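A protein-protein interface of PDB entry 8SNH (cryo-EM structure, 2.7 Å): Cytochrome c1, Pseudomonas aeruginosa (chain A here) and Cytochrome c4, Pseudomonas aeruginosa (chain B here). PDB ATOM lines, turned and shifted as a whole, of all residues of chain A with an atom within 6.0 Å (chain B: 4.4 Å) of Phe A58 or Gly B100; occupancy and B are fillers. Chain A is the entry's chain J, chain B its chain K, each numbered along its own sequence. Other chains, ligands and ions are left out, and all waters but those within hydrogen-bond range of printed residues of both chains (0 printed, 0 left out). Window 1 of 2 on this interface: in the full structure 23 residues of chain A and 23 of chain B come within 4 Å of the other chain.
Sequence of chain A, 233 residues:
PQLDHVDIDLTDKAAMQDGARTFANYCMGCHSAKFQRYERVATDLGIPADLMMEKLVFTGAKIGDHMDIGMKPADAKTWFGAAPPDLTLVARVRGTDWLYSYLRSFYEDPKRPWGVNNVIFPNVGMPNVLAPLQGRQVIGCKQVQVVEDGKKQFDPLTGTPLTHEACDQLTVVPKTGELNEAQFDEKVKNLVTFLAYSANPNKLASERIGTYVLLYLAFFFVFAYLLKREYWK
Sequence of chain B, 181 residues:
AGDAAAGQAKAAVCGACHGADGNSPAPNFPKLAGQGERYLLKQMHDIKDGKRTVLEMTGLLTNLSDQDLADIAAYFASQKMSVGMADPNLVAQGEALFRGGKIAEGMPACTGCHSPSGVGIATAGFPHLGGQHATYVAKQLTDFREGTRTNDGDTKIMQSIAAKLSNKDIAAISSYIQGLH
Phe A58 touches three residues of chain B.
Gly B100 touches just these residues of chain A: Phe A58 (3.2 Å) and Thr A59 (3.7 Å).
Of the printed residues of chain B, Gly A70 touches Lys B102 (3.6 Å).
Of the printed residues of chain A, Lys B102 touches Gly A70 (3.6 Å).
Printed residues of chain A within 4 Å of Ala B96: Phe A58 (3.7 Å).
The nearest residue of chain A that does not touch Gly B100 is Gly A70 (4.1 Å).
Among the printed residues, merely in contact across the chains: Phe A58 with Gly B100 (3.2 Å), Phe A58 with Arg B99 (3.4 Å), Gly A70 with Lys B102 (3.6 Å), Phe A58 with Ala B96 (3.7 Å) and Thr A59 with Gly B100 (3.7 Å).
Of the 15 printed residues of chain A, 3 touch a printed residue of chain B.
Of the 8 printed residues of chain B, 4 touch a printed residue of chain A.
Along chain B the printed residues that touch a printed residue of chain A span positions 96 to 102.
Among the printed residues, 5 pairs touch across the chains.
Among the printed residues, no Asp or Glu carboxylate lies within 4 Å of a Lys or Arg side-chain nitrogen of the other chain.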
ATOM      1  N   ARG A  21     -37.274  22.493 -19.604  1.00  0.00           N
ATOM      2  CA  ARG A  21     -36.593  21.214 -19.421  1.00  0.00           C
ATOM      3  C   ARG A  21     -36.298  20.559 -20.767  1.00  0.00           C
ATOM      4  O   ARG A  21     -35.182  20.078 -21.012  1.00  0.00           O
ATOM      5  CB  ARG A  21     -37.448  20.307 -18.536  1.00  0.00           C
ATOM      6  CG  ARG A  21     -36.871  18.929 -18.273  1.00  0.00           C
ATOM      7  CD  ARG A  21     -37.754  17.844 -18.861  1.00  0.00           C
ATOM      8  NE  ARG A  21     -37.469  16.531 -18.295  1.00  0.00           N
ATOM      9  CZ  ARG A  21     -37.877  15.384 -18.822  1.00  0.00           C
ATOM     10  NH1 ARG A  21     -38.603  15.351 -19.927  1.00  0.00           N
ATOM     11  NH2 ARG A  21     -37.550  14.243 -18.224  1.00  0.00           N
ATOM     12  N   ALA A  24     -33.467  22.472 -22.435  1.00  0.00           N
ATOM     13  CA  ALA A  24     -32.172  22.263 -21.804  1.00  0.00           C
ATOM     14  C   ALA A  24     -31.624  20.874 -22.085  1.00  0.00           C
ATOM     15  O   ALA A  24     -30.403  20.689 -22.115  1.00  0.00           O
ATOM     16  CB  ALA A  24     -32.280  22.488 -20.297  1.00  0.00           C
ATOM     17  N   ASN A  25     -32.497  19.887 -22.287  1.00  0.00           N
ATOM     18  CA  ASN A  25     -32.034  18.516 -22.480  1.00  0.00           C
ATOM     19  C   ASN A  25     -31.856  18.160 -23.954  1.00  0.00           C
ATOM     20  O   ASN A  25     -30.806  17.642 -24.349  1.00  0.00           O
ATOM     21  CB  ASN A  25     -33.007  17.545 -21.807  1.00  0.00           C
ATOM     22  CG  ASN A  25     -32.852  17.524 -20.303  1.00  0.00           C
ATOM     23  OD1 ASN A  25     -31.951  16.879 -19.772  1.00  0.00           O
ATOM     24  ND2 ASN A  25     -33.724  18.238 -19.609  1.00  0.00           N
ATOM     25  N   TYR A  38     -30.052  32.306 -17.231  1.00  0.00           N
ATOM     26  CA  TYR A  38     -30.713  31.303 -16.405  1.00  0.00           C
ATOM     27  C   TYR A  38     -31.458  31.956 -15.251  1.00  0.00           C
ATOM     28  O   TYR A  38     -32.540  31.503 -14.861  1.00  0.00           O
ATOM     29  CB  TYR A  38     -29.695  30.300 -15.860  1.00  0.00           C
ATOM     30  CG  TYR A  38     -29.016  29.434 -16.893  1.00  0.00           C
ATOM     31  CD1 TYR A  38     -29.683  28.371 -17.485  1.00  0.00           C
ATOM     32  CD2 TYR A  38     -27.697  29.664 -17.256  1.00  0.00           C
ATOM     33  CE1 TYR A  38     -29.056  27.568 -18.415  1.00  0.00           C
ATOM     34  CE2 TYR A  38     -27.066  28.871 -18.189  1.00  0.00           C
ATOM     35  CZ  TYR A  38     -27.749  27.824 -18.765  1.00  0.00           C
ATOM     36  OH  TYR A  38     -27.118  27.033 -19.694  1.00  0.00           O
ATOM     37  N   MET A  53     -30.437  25.727 -10.928  1.00  0.00           N
ATOM     38  CA  MET A  53     -29.042  25.312 -10.984  1.00  0.00           C
ATOM     39  C   MET A  53     -28.925  23.802 -11.139  1.00  0.00           C
ATOM     40  O   MET A  53     -28.140  23.311 -11.958  1.00  0.00           O
ATOM     41  CB  MET A  53     -28.322  25.763  -9.710  1.00  0.00           C
ATOM     42  CG  MET A  53     -27.656  27.139  -9.744  1.00  0.00           C
ATOM     43  SD  MET A  53     -27.132  27.728 -11.360  1.00  0.00           S
ATOM     44  CE  MET A  53     -25.474  27.072 -11.381  1.00  0.00           C
ATOM     45  N   GLU A  54     -29.701  23.052 -10.362  1.00  0.00           N
ATOM     46  CA  GLU A  54     -29.549  21.603 -10.331  1.00  0.00           C
ATOM     47  C   GLU A  54     -30.141  20.926 -11.562  1.00  0.00           C
ATOM     48  O   GLU A  54     -29.629  19.888 -11.993  1.00  0.00           O
ATOM     49  CB  GLU A  54     -30.191  21.047  -9.057  1.00  0.00           C
ATOM     50  CG  GLU A  54     -30.594  19.582  -9.123  1.00  0.00           C
ATOM     51  CD  GLU A  54     -31.188  19.085  -7.821  1.00  0.00           C
ATOM     52  OE1 GLU A  54     -32.096  19.757  -7.286  1.00  0.00           O
ATOM     53  OE2 GLU A  54     -30.749  18.024  -7.331  1.00  0.00           O
ATOM     54  N   LYS A  55     -31.204  21.486 -12.139  1.00  0.00           N
ATOM     55  CA  LYS A  55     -32.005  20.771 -13.123  1.00  0.00           C
ATOM     56  C   LYS A  55     -31.833  21.254 -14.553  1.00  0.00           C
ATOM     57  O   LYS A  55     -31.947  20.444 -15.474  1.00  0.00           O
ATOM     58  CB  LYS A  55     -33.492  20.864 -12.756  1.00  0.00           C
ATOM     59  CG  LYS A  55     -33.818  20.413 -11.340  1.00  0.00           C
ATOM     60  CD  LYS A  55     -34.239  18.954 -11.299  1.00  0.00           C
ATOM     61  CE  LYS A  55     -33.860  18.305  -9.980  1.00  0.00           C
ATOM     62  NZ  LYS A  55     -34.710  17.124  -9.667  1.00  0.00           N
ATOM     63  N   LEU A  56     -31.570  22.543 -14.773  1.00  0.00           N
ATOM     64  CA  LEU A  56     -31.537  23.093 -16.121  1.00  0.00           C
ATOM     65  C   LEU A  56     -30.175  23.610 -16.557  1.00  0.00           C
ATOM     66  O   LEU A  56     -29.952  23.739 -17.765  1.00  0.00           O
ATOM     67  CB  LEU A  56     -32.560  24.232 -16.259  1.00  0.00           C
ATOM     68  CG  LEU A  56     -34.026  23.803 -16.147  1.00  0.00           C
ATOM     69  CD1 LEU A  56     -34.950  25.009 -16.133  1.00  0.00           C
ATOM     70  CD2 LEU A  56     -34.399  22.863 -17.275  1.00  0.00           C
ATOM     71  N   VAL A  57     -29.265  23.904 -15.632  1.00  0.00           N
ATOM     72  CA  VAL A  57     -27.938  24.400 -15.978  1.00  0.00           C
ATOM     73  C   VAL A  57     -27.002  23.195 -16.007  1.00  0.00           C
ATOM     74  O   VAL A  57     -26.604  22.676 -14.964  1.00  0.00           O
ATOM     75  CB  VAL A  57     -27.457  25.468 -14.994  1.00  0.00           C
ATOM     76  CG1 VAL A  57     -26.155  26.092 -15.480  1.00  0.00           C
ATOM     77  CG2 VAL A  57     -28.525  26.529 -14.800  1.00  0.00           C
ATOM     78  N   PHE A  58     -26.647  22.751 -17.213  1.00  0.00           N
ATOM     79  CA  PHE A  58     -25.759  21.612 -17.395  1.00  0.00           C
ATOM     80  C   PHE A  58     -24.336  22.012 -17.755  1.00  0.00           C
ATOM     81  O   PHE A  58     -23.442  21.161 -17.712  1.00  0.00           O
ATOM     82  CB  PHE A  58     -26.296  20.689 -18.498  1.00  0.00           C
ATOM     83  CG  PHE A  58     -27.686  20.183 -18.250  1.00  0.00           C
ATOM     84  CD1 PHE A  58     -28.100  19.831 -16.978  1.00  0.00           C
ATOM     85  CD2 PHE A  58     -28.579  20.052 -19.299  1.00  0.00           C
ATOM     86  CE1 PHE A  58     -29.379  19.364 -16.758  1.00  0.00           C
ATOM     87  CE2 PHE A  58     -29.858  19.585 -19.083  1.00  0.00           C
ATOM     88  CZ  PHE A  58     -30.258  19.242 -17.812  1.00  0.00           C
ATOM     89  N   THR A  59     -24.103  23.274 -18.096  1.00  0.00           N
ATOM     90  CA  THR A  59     -22.838  23.710 -18.672  1.00  0.00           C
ATOM     91  C   THR A  59     -21.865  24.257 -17.637  1.00  0.00           C
ATOM     92  O   THR A  59     -20.807  24.772 -18.015  1.00  0.00           O
ATOM     93  CB  THR A  59     -23.095  24.771 -19.743  1.00  0.00           C
ATOM     94  OG1 THR A  59     -23.574  25.972 -19.127  1.00  0.00           O
ATOM     95  CG2 THR A  59     -24.125  24.281 -20.748  1.00  0.00           C
ATOM     96  N   GLY A  60     -22.189  24.165 -16.352  1.00  0.00           N
ATOM     97  CA  GLY A  60     -21.340  24.734 -15.330  1.00  0.00           C
ATOM     98  C   GLY A  60     -21.421  26.238 -15.221  1.00  0.00           C
ATOM     99  O   GLY A  60     -20.650  26.831 -14.459  1.00  0.00           O
ATOM    100  N   ALA A  61     -22.329  26.869 -15.956  1.00  0.00           N
ATOM    101  CA  ALA A  61     -22.498  28.309 -15.885  1.00  0.00           C
ATOM    102  C   ALA A  61     -23.154  28.699 -14.566  1.00  0.00           C
ATOM    103  O   ALA A  61     -23.758  27.877 -13.877  1.00  0.00           O
ATOM    104  CB  ALA A  61     -23.343  28.804 -17.056  1.00  0.00           C
ATOM    105  N   ILE A  69     -23.742  27.551 -24.872  1.00  0.00           N
ATOM    106  CA  ILE A  69     -23.445  26.136 -25.021  1.00  0.00           C
ATOM    107  C   ILE A  69     -22.029  25.995 -25.556  1.00  0.00           C
ATOM    108  O   ILE A  69     -21.428  26.948 -26.055  1.00  0.00           O
ATOM    109  CB  ILE A  69     -24.454  25.422 -25.946  1.00  0.00           C
ATOM    110  CG1 ILE A  69     -24.476  26.067 -27.332  1.00  0.00           C
ATOM    111  CG2 ILE A  69     -25.844  25.465 -25.334  1.00  0.00           C
ATOM    112  CD1 ILE A  69     -25.015  25.160 -28.404  1.00  0.00           C
ATOM    113  N   GLY A  70     -21.494  24.778 -25.437  1.00  0.00           N
ATOM    114  CA  GLY A  70     -20.140  24.515 -25.889  1.00  0.00           C
ATOM    115  C   GLY A  70     -19.980  24.423 -27.391  1.00  0.00           C
ATOM    116  O   GLY A  70     -18.872  24.625 -27.894  1.00  0.00           O
ATOM    117  N   ALA B  96     -21.213  16.126 -16.228  1.00  0.00           N
ATOM    118  CA  ALA B  96     -21.058  17.534 -16.570  1.00  0.00           C
ATOM    119  C   ALA B  96     -20.554  17.685 -17.998  1.00  0.00           C
ATOM    120  O   ALA B  96     -21.077  18.495 -18.771  1.00  0.00           O
ATOM    121  CB  ALA B  96     -20.107  18.212 -15.584  1.00  0.00           C
ATOM    122  N   LEU B  97     -19.549  16.893 -18.374  1.00  0.00           N
ATOM    123  CA  LEU B  97     -19.018  16.978 -19.731  1.00  0.00           C
ATOM    124  C   LEU B  97     -20.058  16.554 -20.762  1.00  0.00           C
ATOM    125  O   LEU B  97     -20.207  17.201 -21.805  1.00  0.00           O
ATOM    126  CB  LEU B  97     -17.760  16.121 -19.854  1.00  0.00           C
ATOM    127  CG  LEU B  97     -16.515  16.692 -19.173  1.00  0.00           C
ATOM    128  CD1 LEU B  97     -15.495  15.598 -18.912  1.00  0.00           C
ATOM    129  CD2 LEU B  97     -15.911  17.801 -20.018  1.00  0.00           C
ATOM    130  N   PHE B  98     -20.786  15.469 -20.492  1.00  0.00           N
ATOM    131  CA  PHE B  98     -21.748  14.955 -21.460  1.00  0.00           C
ATOM    132  C   PHE B  98     -22.893  15.935 -21.676  1.00  0.00           C
ATOM    133  O   PHE B  98     -23.285  16.208 -22.817  1.00  0.00           O
ATOM    134  CB  PHE B  98     -22.280  13.600 -20.991  1.00  0.00           C
ATOM    135  CG  PHE B  98     -22.980  12.814 -22.062  1.00  0.00           C
ATOM    136  CD1 PHE B  98     -24.330  12.998 -22.307  1.00  0.00           C
ATOM    137  CD2 PHE B  98     -22.291  11.881 -22.817  1.00  0.00           C
ATOM    138  CE1 PHE B  98     -24.976  12.275 -23.290  1.00  0.00           C
ATOM    139  CE2 PHE B  98     -22.933  11.155 -23.800  1.00  0.00           C
ATOM    140  CZ  PHE B  98     -24.276  11.352 -24.036  1.00  0.00           C
ATOM    141  N   ARG B  99     -23.445  16.481 -20.591  1.00  0.00           N
ATOM    142  CA  ARG B  99     -24.632  17.319 -20.702  1.00  0.00           C
ATOM    143  C   ARG B  99     -24.301  18.760 -21.066  1.00  0.00           C
ATOM    144  O   ARG B  99     -25.108  19.422 -21.726  1.00  0.00           O
ATOM    145  CB  ARG B  99     -25.421  17.283 -19.394  1.00  0.00           C
ATOM    146  CG  ARG B  99     -25.912  15.902 -19.002  1.00  0.00           C
ATOM    147  CD  ARG B  99     -27.034  15.993 -17.983  1.00  0.00           C
ATOM    148  NE  ARG B  99     -26.632  16.768 -16.816  1.00  0.00           N
ATOM    149  CZ  ARG B  99     -27.242  16.732 -15.640  1.00  0.00           C
ATOM    150  NH1 ARG B  99     -28.300  15.966 -15.432  1.00  0.00           N
ATOM    151  NH2 ARG B  99     -26.782  17.488 -14.649  1.00  0.00           N
ATOM    152  N   GLY B 100     -23.136  19.260 -20.661  1.00  0.00           N
ATOM    153  CA  GLY B 100     -22.823  20.661 -20.847  1.00  0.00           C
ATOM    154  C   GLY B 100     -21.693  20.932 -21.814  1.00  0.00           C
ATOM    155  O   GLY B 100     -21.618  22.019 -22.393  1.00  0.00           O
ATOM    156  N   GLY B 101     -20.804  19.960 -22.000  1.00  0.00           N
ATOM    157  CA  GLY B 101     -19.642  20.199 -22.839  1.00  0.00           C
ATOM    158  C   GLY B 101     -18.644  21.093 -22.130  1.00  0.00           C
ATOM    159  O   GLY B 101     -18.432  20.991 -20.917  1.00  0.00           O
ATOM    160  N   LYS B 102     -18.016  21.984 -22.896  1.00  0.00           N
ATOM    161  CA  LYS B 102     -17.085  22.969 -22.349  1.00  0.00           C
ATOM    162  C   LYS B 102     -17.325  24.292 -23.061  1.00  0.00           C
ATOM    163  O   LYS B 102     -16.934  24.451 -24.222  1.00  0.00           O
ATOM    164  CB  LYS B 102     -15.633  22.523 -22.517  1.00  0.00           C
ATOM    165  CG  LYS B 102     -15.284  21.209 -21.839  1.00  0.00           C
ATOM    166  CD  LYS B 102     -13.866  20.789 -22.192  1.00  0.00           C
ATOM    167  CE  LYS B 102     -13.462  19.499 -21.506  1.00  0.00           C
ATOM    168  NZ  LYS B 102     -12.047  19.143 -21.801  1.00  0.00           N
ATOM    169  N   ALA B 109     -21.630  19.762 -25.990  1.00  0.00           N
ATOM    170  CA  ALA B 109     -22.202  18.692 -25.196  1.00  0.00           C
ATOM    171  C   ALA B 109     -22.522  17.508 -26.098  1.00  0.00           C
ATOM    172  O   ALA B 109     -22.825  17.665 -27.284  1.00  0.00           O
ATOM    173  CB  ALA B 109     -23.465  19.164 -24.479  1.00  0.00           C
